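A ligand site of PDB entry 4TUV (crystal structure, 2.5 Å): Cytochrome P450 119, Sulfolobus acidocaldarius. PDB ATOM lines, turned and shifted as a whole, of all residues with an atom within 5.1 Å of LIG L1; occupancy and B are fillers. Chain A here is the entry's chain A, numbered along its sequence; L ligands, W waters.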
ATOM      1  N   LEU A  33      12.145 -17.041  22.192  1.00  0.00           N
ATOM      2  CA  LEU A  33      12.571 -16.333  20.990  1.00  0.00           C
ATOM      3  C   LEU A  33      13.812 -16.976  20.389  1.00  0.00           C
ATOM      4  O   LEU A  33      13.988 -16.974  19.171  1.00  0.00           O
ATOM      5  CB  LEU A  33      12.859 -14.857  21.288  1.00  0.00           C
ATOM      6  CG  LEU A  33      11.650 -14.033  21.748  1.00  0.00           C
ATOM      7  CD1 LEU A  33      12.095 -12.618  22.040  1.00  0.00           C
ATOM      8  CD2 LEU A  33      10.550 -14.012  20.706  1.00  0.00           C
ATOM      9  N   SER A  41       8.396 -19.799  13.752  1.00  0.00           N
ATOM     10  CA  SER A  41       7.857 -18.550  13.247  1.00  0.00           C
ATOM     11  C   SER A  41       7.071 -18.806  11.963  1.00  0.00           C
ATOM     12  O   SER A  41       6.469 -17.885  11.398  1.00  0.00           O
ATOM     13  CB  SER A  41       8.977 -17.544  12.959  1.00  0.00           C
ATOM     14  OG  SER A  41       9.474 -16.942  14.137  1.00  0.00           O
ATOM     15  N   MET A  68      10.830 -13.317   5.474  1.00  0.00           N
ATOM     16  CA  MET A  68      11.720 -13.812   6.517  1.00  0.00           C
ATOM     17  C   MET A  68      11.050 -13.840   7.881  1.00  0.00           C
ATOM     18  O   MET A  68      11.324 -14.719   8.702  1.00  0.00           O
ATOM     19  CB  MET A  68      12.993 -12.965   6.576  1.00  0.00           C
ATOM     20  CG  MET A  68      12.831 -11.533   7.131  1.00  0.00           C
ATOM     21  SD  MET A  68      14.397 -10.594   7.073  1.00  0.00           S
ATOM     22  CE  MET A  68      14.453 -10.244   5.323  1.00  0.00           C
ATOM     23  N   LEU A  69      10.156 -12.891   8.117  1.00  0.00           N
ATOM     24  CA  LEU A  69       9.442 -12.751   9.378  1.00  0.00           C
ATOM     25  C   LEU A  69       8.647 -14.012   9.783  1.00  0.00           C
ATOM     26  O   LEU A  69       8.580 -14.370  10.958  1.00  0.00           O
ATOM     27  CB  LEU A  69       8.501 -11.545   9.277  1.00  0.00           C
ATOM     28  CG  LEU A  69       7.724 -11.077  10.504  1.00  0.00           C
ATOM     29  CD1 LEU A  69       8.639 -10.607  11.636  1.00  0.00           C
ATOM     30  CD2 LEU A  69       6.823  -9.962  10.038  1.00  0.00           C
ATOM     31  N   HIS A  76      14.691 -18.777   6.267  1.00  0.00           N
ATOM     32  CA  HIS A  76      14.876 -17.487   6.916  1.00  0.00           C
ATOM     33  C   HIS A  76      16.263 -16.879   6.723  1.00  0.00           C
ATOM     34  O   HIS A  76      16.385 -15.708   6.386  1.00  0.00           O
ATOM     35  CB  HIS A  76      14.622 -17.606   8.405  1.00  0.00           C
ATOM     36  CG  HIS A  76      15.031 -16.386   9.162  1.00  0.00           C
ATOM     37  ND1 HIS A  76      16.261 -16.258   9.749  1.00  0.00           N
ATOM     38  CD2 HIS A  76      14.380 -15.221   9.404  1.00  0.00           C
ATOM     39  CE1 HIS A  76      16.357 -15.085  10.341  1.00  0.00           C
ATOM     40  NE2 HIS A  76      15.218 -14.436  10.147  1.00  0.00           N
ATOM     41  N   ARG A  80      17.186 -13.528   4.727  1.00  0.00           N
ATOM     42  CA  ARG A  80      17.694 -12.362   5.407  1.00  0.00           C
ATOM     43  C   ARG A  80      19.092 -12.002   4.911  1.00  0.00           C
ATOM     44  O   ARG A  80      19.492 -10.840   4.966  1.00  0.00           O
ATOM     45  CB  ARG A  80      17.726 -12.570   6.919  1.00  0.00           C
ATOM     46  CG  ARG A  80      18.289 -11.381   7.677  1.00  0.00           C
ATOM     47  CD  ARG A  80      17.757 -11.314   9.091  1.00  0.00           C
ATOM     48  NE  ARG A  80      18.499 -10.358   9.912  1.00  0.00           N
ATOM     49  CZ  ARG A  80      18.119  -9.933  11.110  1.00  0.00           C
ATOM     50  NH1 ARG A  80      16.959 -10.344  11.628  1.00  0.00           N
ATOM     51  NH2 ARG A  80      18.880  -9.075  11.772  1.00  0.00           N
ATOM     52  N   PHE A  87      21.531  -3.118   6.249  1.00  0.00           N
ATOM     53  CA  PHE A  87      20.918  -2.616   7.475  1.00  0.00           C
ATOM     54  C   PHE A  87      21.830  -2.750   8.677  1.00  0.00           C
ATOM     55  O   PHE A  87      21.393  -2.640   9.816  1.00  0.00           O
ATOM     56  CB  PHE A  87      19.594  -3.329   7.728  1.00  0.00           C
ATOM     57  CG  PHE A  87      18.534  -3.001   6.718  1.00  0.00           C
ATOM     58  CD1 PHE A  87      17.665  -1.933   6.919  1.00  0.00           C
ATOM     59  CD2 PHE A  87      18.439  -3.737   5.536  1.00  0.00           C
ATOM     60  CE1 PHE A  87      16.691  -1.599   5.979  1.00  0.00           C
ATOM     61  CE2 PHE A  87      17.472  -3.405   4.580  1.00  0.00           C
ATOM     62  CZ  PHE A  87      16.593  -2.342   4.809  1.00  0.00           C
ATOM     63  N   ILE A 130      13.555   5.349   4.520  1.00  0.00           N
ATOM     64  CA  ILE A 130      13.496   4.038   3.878  1.00  0.00           C
ATOM     65  C   ILE A 130      13.332   4.216   2.362  1.00  0.00           C
ATOM     66  O   ILE A 130      13.862   3.429   1.571  1.00  0.00           O
ATOM     67  CB  ILE A 130      12.348   3.158   4.463  1.00  0.00           C
ATOM     68  CG1 ILE A 130      12.546   1.701   4.080  1.00  0.00           C
ATOM     69  CG2 ILE A 130      10.969   3.656   4.067  1.00  0.00           C
ATOM     70  CD1 ILE A 130      13.699   1.069   4.779  1.00  0.00           C
ATOM     71  N   LEU A 205       7.697  -5.657   2.695  1.00  0.00           N
ATOM     72  CA  LEU A 205       8.168  -5.769   4.060  1.00  0.00           C
ATOM     73  C   LEU A 205       9.188  -4.688   4.386  1.00  0.00           C
ATOM     74  O   LEU A 205       8.992  -3.936   5.335  1.00  0.00           O
ATOM     75  CB  LEU A 205       8.770  -7.157   4.305  1.00  0.00           C
ATOM     76  CG  LEU A 205       9.203  -7.393   5.756  1.00  0.00           C
ATOM     77  CD1 LEU A 205       8.002  -7.616   6.660  1.00  0.00           C
ATOM     78  CD2 LEU A 205      10.187  -8.525   5.861  1.00  0.00           C
ATOM     79  N   LEU A 206      10.263  -4.584   3.605  1.00  0.00           N
ATOM     80  CA  LEU A 206      11.297  -3.588   3.871  1.00  0.00           C
ATOM     81  C   LEU A 206      10.777  -2.150   3.777  1.00  0.00           C
ATOM     82  O   LEU A 206      11.138  -1.290   4.586  1.00  0.00           O
ATOM     83  CB  LEU A 206      12.475  -3.774   2.916  1.00  0.00           C
ATOM     84  CG  LEU A 206      13.233  -5.084   3.024  1.00  0.00           C
ATOM     85  CD1 LEU A 206      14.414  -5.113   2.065  1.00  0.00           C
ATOM     86  CD2 LEU A 206      13.681  -5.264   4.444  1.00  0.00           C
ATOM     87  N   GLY A 210       8.372  -1.152   8.787  1.00  0.00           N
ATOM     88  CA  GLY A 210       9.123  -0.489   9.830  1.00  0.00           C
ATOM     89  C   GLY A 210       8.728   0.955  10.109  1.00  0.00           C
ATOM     90  O   GLY A 210       9.172   1.559  11.073  1.00  0.00           O
ATOM     91  N   THR A 213       6.387   1.499  13.472  1.00  0.00           N
ATOM     92  CA  THR A 213       7.120   1.110  14.681  1.00  0.00           C
ATOM     93  C   THR A 213       8.181   2.153  15.023  1.00  0.00           C
ATOM     94  O   THR A 213       8.302   2.561  16.179  1.00  0.00           O
ATOM     95  CB  THR A 213       7.805  -0.272  14.536  1.00  0.00           C
ATOM     96  OG1 THR A 213       8.637  -0.268  13.380  1.00  0.00           O
ATOM     97  CG2 THR A 213       6.777  -1.378  14.394  1.00  0.00           C
ATOM     98  N   THR A 214       8.954   2.568  14.022  1.00  0.00           N
ATOM     99  CA  THR A 214       9.963   3.611  14.207  1.00  0.00           C
ATOM    100  C   THR A 214       9.283   4.931  14.603  1.00  0.00           C
ATOM    101  O   THR A 214       9.757   5.655  15.484  1.00  0.00           O
ATOM    102  CB  THR A 214      10.795   3.814  12.920  1.00  0.00           C
ATOM    103  OG1 THR A 214      11.413   2.589  12.543  1.00  0.00           O
ATOM    104  CG2 THR A 214      11.854   4.863  13.114  1.00  0.00           C
ATOM    105  N   LEU A 217       8.529   4.758  18.156  1.00  0.00           N
ATOM    106  CA  LEU A 217       9.700   4.934  19.029  1.00  0.00           C
ATOM    107  C   LEU A 217       9.963   6.413  19.272  1.00  0.00           C
ATOM    108  O   LEU A 217      10.181   6.833  20.412  1.00  0.00           O
ATOM    109  CB  LEU A 217      10.935   4.278  18.428  1.00  0.00           C
ATOM    110  CG  LEU A 217      12.291   4.579  19.089  1.00  0.00           C
ATOM    111  CD1 LEU A 217      12.271   4.291  20.600  1.00  0.00           C
ATOM    112  CD2 LEU A 217      13.406   3.779  18.406  1.00  0.00           C
ATOM    113  N   LEU A 248      12.976   2.384  24.590  1.00  0.00           N
ATOM    114  CA  LEU A 248      12.665   1.106  23.954  1.00  0.00           C
ATOM    115  C   LEU A 248      12.227   0.085  25.003  1.00  0.00           C
ATOM    116  O   LEU A 248      11.232  -0.597  24.807  1.00  0.00           O
ATOM    117  CB  LEU A 248      13.858   0.581  23.172  1.00  0.00           C
ATOM    118  CG  LEU A 248      14.062   1.220  21.810  1.00  0.00           C
ATOM    119  CD1 LEU A 248      15.532   1.194  21.436  1.00  0.00           C
ATOM    120  CD2 LEU A 248      13.231   0.495  20.751  1.00  0.00           C
ATOM    121  N   PRO A 253       7.558  -0.204  21.107  1.00  0.00           N
ATOM    122  CA  PRO A 253       6.641  -0.025  19.987  1.00  0.00           C
ATOM    123  C   PRO A 253       5.963  -1.320  19.546  1.00  0.00           C
ATOM    124  O   PRO A 253       4.839  -1.269  18.997  1.00  0.00           O
ATOM    125  CB  PRO A 253       7.532   0.525  18.870  1.00  0.00           C
ATOM    126  CG  PRO A 253       8.658   1.155  19.574  1.00  0.00           C
ATOM    127  CD  PRO A 253       8.904   0.303  20.787  1.00  0.00           C
ATOM    128  N   VAL A 254       6.619  -2.450  19.759  1.00  0.00           N
ATOM    129  CA  VAL A 254       5.992  -3.748  19.556  1.00  0.00           C
ATOM    130  C   VAL A 254       5.831  -4.423  20.911  1.00  0.00           C
ATOM    131  O   VAL A 254       6.811  -4.706  21.581  1.00  0.00           O
ATOM    132  CB  VAL A 254       6.801  -4.630  18.583  1.00  0.00           C
ATOM    133  CG1 VAL A 254       6.077  -5.960  18.309  1.00  0.00           C
ATOM    134  CG2 VAL A 254       7.029  -3.882  17.288  1.00  0.00           C
ATOM    135  N   THR A 257       5.039 -10.704  20.544  1.00  0.00           N
ATOM    136  CA  THR A 257       5.155 -11.474  19.345  1.00  0.00           C
ATOM    137  C   THR A 257       4.632 -12.875  19.665  1.00  0.00           C
ATOM    138  O   THR A 257       4.316 -13.179  20.824  1.00  0.00           O
ATOM    139  CB  THR A 257       6.614 -11.499  18.826  1.00  0.00           C
ATOM    140  OG1 THR A 257       6.657 -12.000  17.481  1.00  0.00           O
ATOM    141  CG2 THR A 257       7.443 -12.378  19.671  1.00  0.00           C
ATOM    142  N   VAL A 258       4.538 -13.744  18.651  1.00  0.00           N
ATOM    143  CA  VAL A 258       3.964 -15.058  18.855  1.00  0.00           C
ATOM    144  C   VAL A 258       4.782 -16.152  18.132  1.00  0.00           C
ATOM    145  O   VAL A 258       5.497 -15.877  17.179  1.00  0.00           O
ATOM    146  CB  VAL A 258       2.488 -15.064  18.392  1.00  0.00           C
ATOM    147  CG1 VAL A 258       2.379 -14.571  16.959  1.00  0.00           C
ATOM    148  CG2 VAL A 258       1.842 -16.435  18.577  1.00  0.00           C
ATOM    149  N   ARG A 259       4.721 -17.380  18.655  1.00  0.00           N
ATOM    150  CA  ARG A 259       5.318 -18.544  18.014  1.00  0.00           C
ATOM    151  C   ARG A 259       4.329 -19.721  18.044  1.00  0.00           C
ATOM    152  O   ARG A 259       3.336 -19.703  18.783  1.00  0.00           O
ATOM    153  CB  ARG A 259       6.619 -18.936  18.707  1.00  0.00           C
ATOM    154  CG  ARG A 259       7.708 -17.875  18.690  1.00  0.00           C
ATOM    155  CD  ARG A 259       8.420 -17.825  17.343  1.00  0.00           C
ATOM    156  NE  ARG A 259       9.558 -16.909  17.385  1.00  0.00           N
ATOM    157  CZ  ARG A 259       9.485 -15.608  17.124  1.00  0.00           C
ATOM    158  NH1 ARG A 259       8.321 -15.051  16.797  1.00  0.00           N
ATOM    159  NH2 ARG A 259      10.571 -14.855  17.193  1.00  0.00           N
ATOM    160  N   ILE A 282       6.783  -9.125  25.235  1.00  0.00           N
ATOM    161  CA  ILE A 282       7.991  -8.299  25.255  1.00  0.00           C
ATOM    162  C   ILE A 282       7.927  -7.200  26.311  1.00  0.00           C
ATOM    163  O   ILE A 282       8.866  -7.010  27.093  1.00  0.00           O
ATOM    164  CB  ILE A 282       8.221  -7.646  23.858  1.00  0.00           C
ATOM    165  CG1 ILE A 282       8.666  -8.711  22.846  1.00  0.00           C
ATOM    166  CG2 ILE A 282       9.260  -6.527  23.927  1.00  0.00           C
ATOM    167  CD1 ILE A 282       8.805  -8.190  21.424  1.00  0.00           C
ATOM    168  N   LEU A 308      14.122  -6.503  25.209  1.00  0.00           N
ATOM    169  CA  LEU A 308      13.720  -7.409  24.146  1.00  0.00           C
ATOM    170  C   LEU A 308      12.891  -6.746  23.047  1.00  0.00           C
ATOM    171  O   LEU A 308      12.190  -7.435  22.296  1.00  0.00           O
ATOM    172  CB  LEU A 308      12.949  -8.587  24.729  1.00  0.00           C
ATOM    173  CG  LEU A 308      13.744  -9.430  25.727  1.00  0.00           C
ATOM    174  CD1 LEU A 308      12.925 -10.596  26.211  1.00  0.00           C
ATOM    175  CD2 LEU A 308      15.065  -9.897  25.097  1.00  0.00           C
ATOM    176  N   SER A 309      12.986  -5.424  22.954  1.00  0.00           N
ATOM    177  CA  SER A 309      12.056  -4.661  22.116  1.00  0.00           C
ATOM    178  C   SER A 309      12.272  -4.842  20.607  1.00  0.00           C
ATOM    179  O   SER A 309      11.372  -4.597  19.804  1.00  0.00           O
ATOM    180  CB  SER A 309      12.134  -3.184  22.505  1.00  0.00           C
ATOM    181  OG  SER A 309      11.821  -3.056  23.882  1.00  0.00           O
ATOM    182  N   PHE A 310      13.460  -5.303  20.235  1.00  0.00           N
ATOM    183  CA  PHE A 310      13.728  -5.760  18.870  1.00  0.00           C
ATOM    184  C   PHE A 310      13.739  -7.282  18.748  1.00  0.00           C
ATOM    185  O   PHE A 310      14.194  -7.827  17.736  1.00  0.00           O
ATOM    186  CB  PHE A 310      15.084  -5.229  18.399  1.00  0.00           C
ATOM    187  CG  PHE A 310      15.123  -3.752  18.218  1.00  0.00           C
ATOM    188  CD1 PHE A 310      14.341  -3.124  17.271  1.00  0.00           C
ATOM    189  CD2 PHE A 310      15.983  -2.983  18.992  1.00  0.00           C
ATOM    190  CE1 PHE A 310      14.402  -1.766  17.089  1.00  0.00           C
ATOM    191  CE2 PHE A 310      16.049  -1.605  18.823  1.00  0.00           C
ATOM    192  CZ  PHE A 310      15.255  -0.995  17.879  1.00  0.00           C
ATOM    193  N   GLY A 311      13.252  -7.964  19.780  1.00  0.00           N
ATOM    194  CA  GLY A 311      13.289  -9.418  19.820  1.00  0.00           C
ATOM    195  C   GLY A 311      14.634  -9.994  20.230  1.00  0.00           C
ATOM    196  O   GLY A 311      15.439  -9.321  20.851  1.00  0.00           O
ATOM    197  N   ILE A 314      17.485 -15.255  16.024  1.00  0.00           N
ATOM    198  CA  ILE A 314      17.685 -15.135  14.587  1.00  0.00           C
ATOM    199  C   ILE A 314      16.740 -14.127  13.948  1.00  0.00           C
ATOM    200  O   ILE A 314      16.967 -13.697  12.818  1.00  0.00           O
ATOM    201  CB  ILE A 314      17.479 -16.490  13.854  1.00  0.00           C
ATOM    202  CG1 ILE A 314      16.039 -16.969  14.046  1.00  0.00           C
ATOM    203  CG2 ILE A 314      18.450 -17.548  14.363  1.00  0.00           C
ATOM    204  CD1 ILE A 314      15.713 -18.192  13.244  1.00  0.00           C
ATOM    205  N   HIS A 315      15.671 -13.746  14.643  1.00  0.00           N
ATOM    206  CA  HIS A 315      14.720 -12.812  14.062  1.00  0.00           C
ATOM    207  C   HIS A 315      14.928 -11.383  14.578  1.00  0.00           C
ATOM    208  O   HIS A 315      14.185 -10.465  14.205  1.00  0.00           O
ATOM    209  CB  HIS A 315      13.289 -13.280  14.321  1.00  0.00           C
ATOM    210  CG  HIS A 315      12.875 -14.450  13.474  1.00  0.00           C
ATOM    211  ND1 HIS A 315      12.507 -14.315  12.152  1.00  0.00           N
ATOM    212  CD2 HIS A 315      12.774 -15.775  13.755  1.00  0.00           C
ATOM    213  CE1 HIS A 315      12.201 -15.502  11.659  1.00  0.00           C
ATOM    214  NE2 HIS A 315      12.353 -16.397  12.612  1.00  0.00           N
ATOM    215  N   LEU A 316      15.933 -11.217  15.423  1.00  0.00           N
ATOM    216  CA  LEU A 316      16.272  -9.900  15.972  1.00  0.00           C
ATOM    217  C   LEU A 316      16.187  -8.801  14.910  1.00  0.00           C
ATOM    218  O   LEU A 316      16.945  -8.823  13.928  1.00  0.00           O
ATOM    219  CB  LEU A 316      17.663  -9.908  16.570  1.00  0.00           C
ATOM    220  CG  LEU A 316      18.113  -8.530  17.060  1.00  0.00           C
ATOM    221  CD1 LEU A 316      17.458  -8.234  18.392  1.00  0.00           C
ATOM    222  CD2 LEU A 316      19.638  -8.478  17.171  1.00  0.00           C
ATOM    223  N   CYS A 317      15.262  -7.872  15.135  1.00  0.00           N
ATOM    224  CA  CYS A 317      14.843  -6.871  14.140  1.00  0.00           C
ATOM    225  C   CYS A 317      15.947  -6.427  13.174  1.00  0.00           C
ATOM    226  O   CYS A 317      16.983  -5.877  13.575  1.00  0.00           O
ATOM    227  CB  CYS A 317      14.260  -5.653  14.832  1.00  0.00           C
ATOM    228  SG  CYS A 317      13.789  -4.332  13.668  1.00  0.00           S
ATOM    229  N   LEU A 318      15.695  -6.676  11.904  1.00  0.00           N
ATOM    230  CA  LEU A 318      16.565  -6.232  10.821  1.00  0.00           C
ATOM    231  C   LEU A 318      16.717  -4.716  10.819  1.00  0.00           C
ATOM    232  O   LEU A 318      17.759  -4.202  10.433  1.00  0.00           O
ATOM    233  CB  LEU A 318      16.015  -6.713   9.477  1.00  0.00           C
ATOM    234  CG  LEU A 318      16.832  -6.418   8.230  1.00  0.00           C
ATOM    235  CD1 LEU A 318      18.225  -7.023   8.353  1.00  0.00           C
ATOM    236  CD2 LEU A 318      16.105  -6.932   6.952  1.00  0.00           C
ATOM    237  N   GLY A 319      15.679  -3.993  11.246  1.00  0.00           N
ATOM    238  CA  GLY A 319      15.711  -2.542  11.250  1.00  0.00           C
ATOM    239  C   GLY A 319      16.256  -1.899  12.515  1.00  0.00           C
ATOM    240  O   GLY A 319      16.258  -0.680  12.646  1.00  0.00           O
ATOM    241  N   ALA A 320      16.698  -2.712  13.479  1.00  0.00           N
ATOM    242  CA  ALA A 320      17.115  -2.139  14.752  1.00  0.00           C
ATOM    243  C   ALA A 320      18.219  -1.080  14.623  1.00  0.00           C
ATOM    244  O   ALA A 320      18.117  -0.005  15.220  1.00  0.00           O
ATOM    245  CB  ALA A 320      17.545  -3.239  15.720  1.00  0.00           C
ATOM    246  N   LEU A 322      18.890   0.762  12.037  1.00  0.00           N
ATOM    247  CA  LEU A 322      18.229   1.885  11.385  1.00  0.00           C
ATOM    248  C   LEU A 322      17.305   2.657  12.340  1.00  0.00           C
ATOM    249  O   LEU A 322      17.406   3.881  12.419  1.00  0.00           O
ATOM    250  CB  LEU A 322      17.439   1.382  10.179  1.00  0.00           C
ATOM    251  CG  LEU A 322      16.747   2.482   9.388  1.00  0.00           C
ATOM    252  CD1 LEU A 322      17.719   3.628   9.094  1.00  0.00           C
ATOM    253  CD2 LEU A 322      16.134   1.923   8.108  1.00  0.00           C
ATOM    254  N   ALA A 323      16.422   1.960  13.052  1.00  0.00           N
ATOM    255  CA  ALA A 323      15.494   2.614  14.006  1.00  0.00           C
ATOM    256  C   ALA A 323      16.239   3.351  15.114  1.00  0.00           C
ATOM    257  O   ALA A 323      15.889   4.488  15.442  1.00  0.00           O
ATOM    258  CB  ALA A 323      14.526   1.591  14.636  1.00  0.00           C
HETATM  259  C1  LIG L   1      10.556  -4.509  16.492  1.00  0.00           C
HETATM  260  C2  LIG L   1      11.850  -1.169  13.252  1.00  0.00           C
HETATM  261  C3  LIG L   1      11.886  -4.649   9.921  1.00  0.00           C
HETATM  262  C4  LIG L   1      11.223  -7.402  14.554  1.00  0.00           C
HETATM  263  C5  LIG L   1      10.891  -7.995  15.822  1.00  0.00           C
HETATM  264  C6  LIG L   1      10.615  -7.004  16.657  1.00  0.00           C
HETATM  265  C7  LIG L   1      10.752  -5.751  15.936  1.00  0.00           C
HETATM  266  C8  LIG L   1      10.196  -7.126  18.131  1.00  0.00           C
HETATM  267  C9  LIG L   1      10.876  -9.507  16.132  1.00  0.00           C
HETATM  268  C10 LIG L   1       9.653 -10.189  15.504  1.00  0.00           C
HETATM  269  C11 LIG L   1       9.674 -11.661  15.838  1.00  0.00           C
HETATM  270  O1  LIG L   1      10.631 -12.138  16.502  1.00  0.00           O
HETATM  271  O2  LIG L   1       8.709 -12.378  15.456  1.00  0.00           O
HETATM  272  C12 LIG L   1      10.866  -3.304  15.911  1.00  0.00           C
HETATM  273  C13 LIG L   1      10.837  -2.025  16.593  1.00  0.00           C
HETATM  274  C14 LIG L   1      11.179  -1.103  15.678  1.00  0.00           C
HETATM  275  C15 LIG L   1      11.445  -1.772  14.420  1.00  0.00           C
HETATM  276  C16 LIG L   1      10.456  -1.832  18.078  1.00  0.00           C
HETATM  277  C17 LIG L   1      11.336   0.421  15.849  1.00  0.00           C
HETATM  278  C18 LIG L   1      11.433   1.022  17.047  1.00  0.00           C
HETATM  279  C19 LIG L   1      12.015  -1.828  12.062  1.00  0.00           C
HETATM  280  C20 LIG L   1      12.458  -1.250  10.800  1.00  0.00           C
HETATM  281  C21 LIG L   1      12.466  -2.254   9.898  1.00  0.00           C
HETATM  282  C22 LIG L   1      12.006  -3.449  10.552  1.00  0.00           C
HETATM  283  C23 LIG L   1      12.875   0.229  10.577  1.00  0.00           C
HETATM  284  C24 LIG L   1      12.813  -2.278   8.398  1.00  0.00           C
HETATM  285  C25 LIG L   1      12.870  -1.212   7.599  1.00  0.00           C
HETATM  286  C26 LIG L   1      11.893  -5.901  10.484  1.00  0.00           C
HETATM  287  C27 LIG L   1      12.127  -7.128   9.771  1.00  0.00           C
HETATM  288  C28 LIG L   1      12.042  -8.127  10.657  1.00  0.00           C
HETATM  289  C29 LIG L   1      11.747  -7.555  11.946  1.00  0.00           C
HETATM  290  C30 LIG L   1      12.433  -7.294   8.262  1.00  0.00           C
HETATM  291  C31 LIG L   1      12.220  -9.611  10.395  1.00  0.00           C
HETATM  292  C32 LIG L   1      13.631 -10.008  10.806  1.00  0.00           C
HETATM  293  C33 LIG L   1      13.793 -11.505  10.666  1.00  0.00           C
HETATM  294  O3  LIG L   1      12.781 -12.234  10.480  1.00  0.00           O
HETATM  295  O4  LIG L   1      14.945 -11.999  10.758  1.00  0.00           O
HETATM  296  N1  LIG L   1      11.136  -6.025  14.640  1.00  0.00           N
HETATM  297  N2  LIG L   1      11.237  -3.133  14.601  1.00  0.00           N
HETATM  298  N3  LIG L   1      11.730  -3.174  11.871  1.00  0.00           N
HETATM  299  N4  LIG L   1      11.648  -6.182  11.818  1.00  0.00           N
HETATM  300 FE1  LIG L   1      11.528  -4.596  13.205  1.00  0.00          FE
HETATM  301  C1  LG2 L   2       5.771  -6.199  14.258  1.00  0.00           C
HETATM  302  C2  LG2 L   2       4.445  -6.549  14.612  1.00  0.00           C
HETATM  303  C3  LG2 L   2       3.395  -5.873  14.018  1.00  0.00           C
HETATM  304  C4  LG2 L   2       3.622  -4.845  13.096  1.00  0.00           C
HETATM  305  C5  LG2 L   2       4.932  -4.505  12.748  1.00  0.00           C
HETATM  306  C6  LG2 L   2       5.988  -5.183  13.327  1.00  0.00           C
HETATM  307  C7  LG2 L   2       7.360  -4.826  12.972  1.00  0.00           C
HETATM  308  C8  LG2 L   2       8.587  -5.231  13.494  1.00  0.00           C
HETATM  309  N1  LG2 L   2       9.659  -4.621  12.812  1.00  0.00           N
HETATM  310  C9  LG2 L   2       9.047  -3.834  11.877  1.00  0.00           C
HETATM  311  N2  LG2 L   2       7.674  -3.929  11.952  1.00  0.00           N
HETATM  312 CL1  LG2 L   2       1.738  -6.308  14.464  1.00  0.00          CL
HETATM  313  O   HOH W   1       9.093  -3.301  20.910  1.00  0.00           O
HETATM  314  O   HOH W   2       6.118 -10.851  14.466  1.00  0.00           O
HETATM  315  O   HOH W   3       9.640 -14.495  13.817  1.00  0.00           O
HETATM  316  O   HOH W   4      13.168 -12.111  17.795  1.00  0.00           O
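An iron atom (FE1) of LIG L1 is bound by the side-chain sulfur (SG) of Cys 317, 2.3 Å away.
An oxygen (O4) of LIG L1 is in hydrogen-bond range of a ring nitrogen (NE2) of His 76, 2.5 Å away.
ND1 of His 315 sits at hydrogen-bond distance from O3 of LIG L1 (2.7 Å).
The guanidinium group (NH1) of Arg 80 is in salt-bridge range of an oxygen (O4) of LIG L1 (2.7 Å).
An oxygen (O1) of LIG L1 is in salt-bridge range of the guanidinium group (NH2) of Arg 259.
The side-chain hydroxyl (OG1) of Thr 257 is in hydrogen-bond range of an oxygen (O2) of LIG L1 (2.9 Å).
A nitrogen (N1) of LG2 L2 binds an iron atom (FE1) of LIG L1, 1.9 Å away.
The side-chain sulfur (SG) of Cys 317 lies close to the backbone NH (N) of Gly 319 (3.1 Å).
The backbone carbonyl oxygen of Phe 310 lies within hydrogen-bond range of the backbone NH of Cys 317 (2.8 Å).
A ring nitrogen (NE2) of His 76 lies within hydrogen-bond range of a ring nitrogen (ND1) of His 315 (3.4 Å).
A ring nitrogen (NE2) of His 76 lies close to the backbone carbonyl oxygen of Ile 314 (3.3 Å).
A ring nitrogen (NE2) of His 315 sits at hydrogen-bond distance from the side-chain hydroxyl of Ser 41 (3.3 Å).
The side-chain hydroxyl of Ser 41 sits at hydrogen-bond distance from the guanidinium group of Arg 259, at 3.2 Å.
OG of Ser 309 is in hydrogen-bond range of O of Leu 248 (2.7 Å).
The backbone carbonyl oxygen of Gly 210 is in hydrogen-bond range of the side-chain hydroxyl of Thr 213, at 3.0 Å.
O3 of LIG L1 lies close to O of Met 68.
An oxygen (O4) of LIG L1 sits close to the backbone carbonyl oxygen (O) of Ile 314 (3.3 Å).
Residues that only touch LIG L1: Leu 69 (3.6 Å), Ile 130 (3.7 Å), Leu 205 (3.5 Å), Leu 206 (3.5 Å), Gly 210 (3.6 Å), Thr 213 (3.3 Å), Thr 214 (3.4 Å), Leu 217 (3.6 Å), Pro 253 (3.8 Å), Val 254 (3.7 Å), Ile 282 (3.7 Å), Ser 309 (3.3 Å), Phe 310 (3.6 Å), Gly 311 (3.6 Å), Leu 318 (3.8 Å), Gly 319 (3.5 Å) and Ala 323 (3.6 Å).
Hydrophobic or aromatic side chains that line LIG L1: Met 68, Leu 69, His 76, Ile 130, Leu 205, Leu 217, Pro 253, Val 254, Ile 282, Phe 310, His 315, Leu 318 and Ala 323.
Of the 34 residues printed, 25 come within 4 Å of LIG L1.
Water W3 lies within hydrogen-bond range of OG of Ser 41 (2.5 Å), O2 of LIG L1 (2.8 Å), O of Leu 69 (3.1 Å), NH1 of Arg 259 (3.3 Å) and ND1 of His 315 (3.3 Å).
Water W2 lies within hydrogen-bond range of O2 of LIG L1 (3.2 Å) and OG1 of Thr 257 (3.3 Å).
Water W1 lies within hydrogen-bond range of O of Val 254 (2.8 Å) and O of Ser 309 (2.8 Å).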
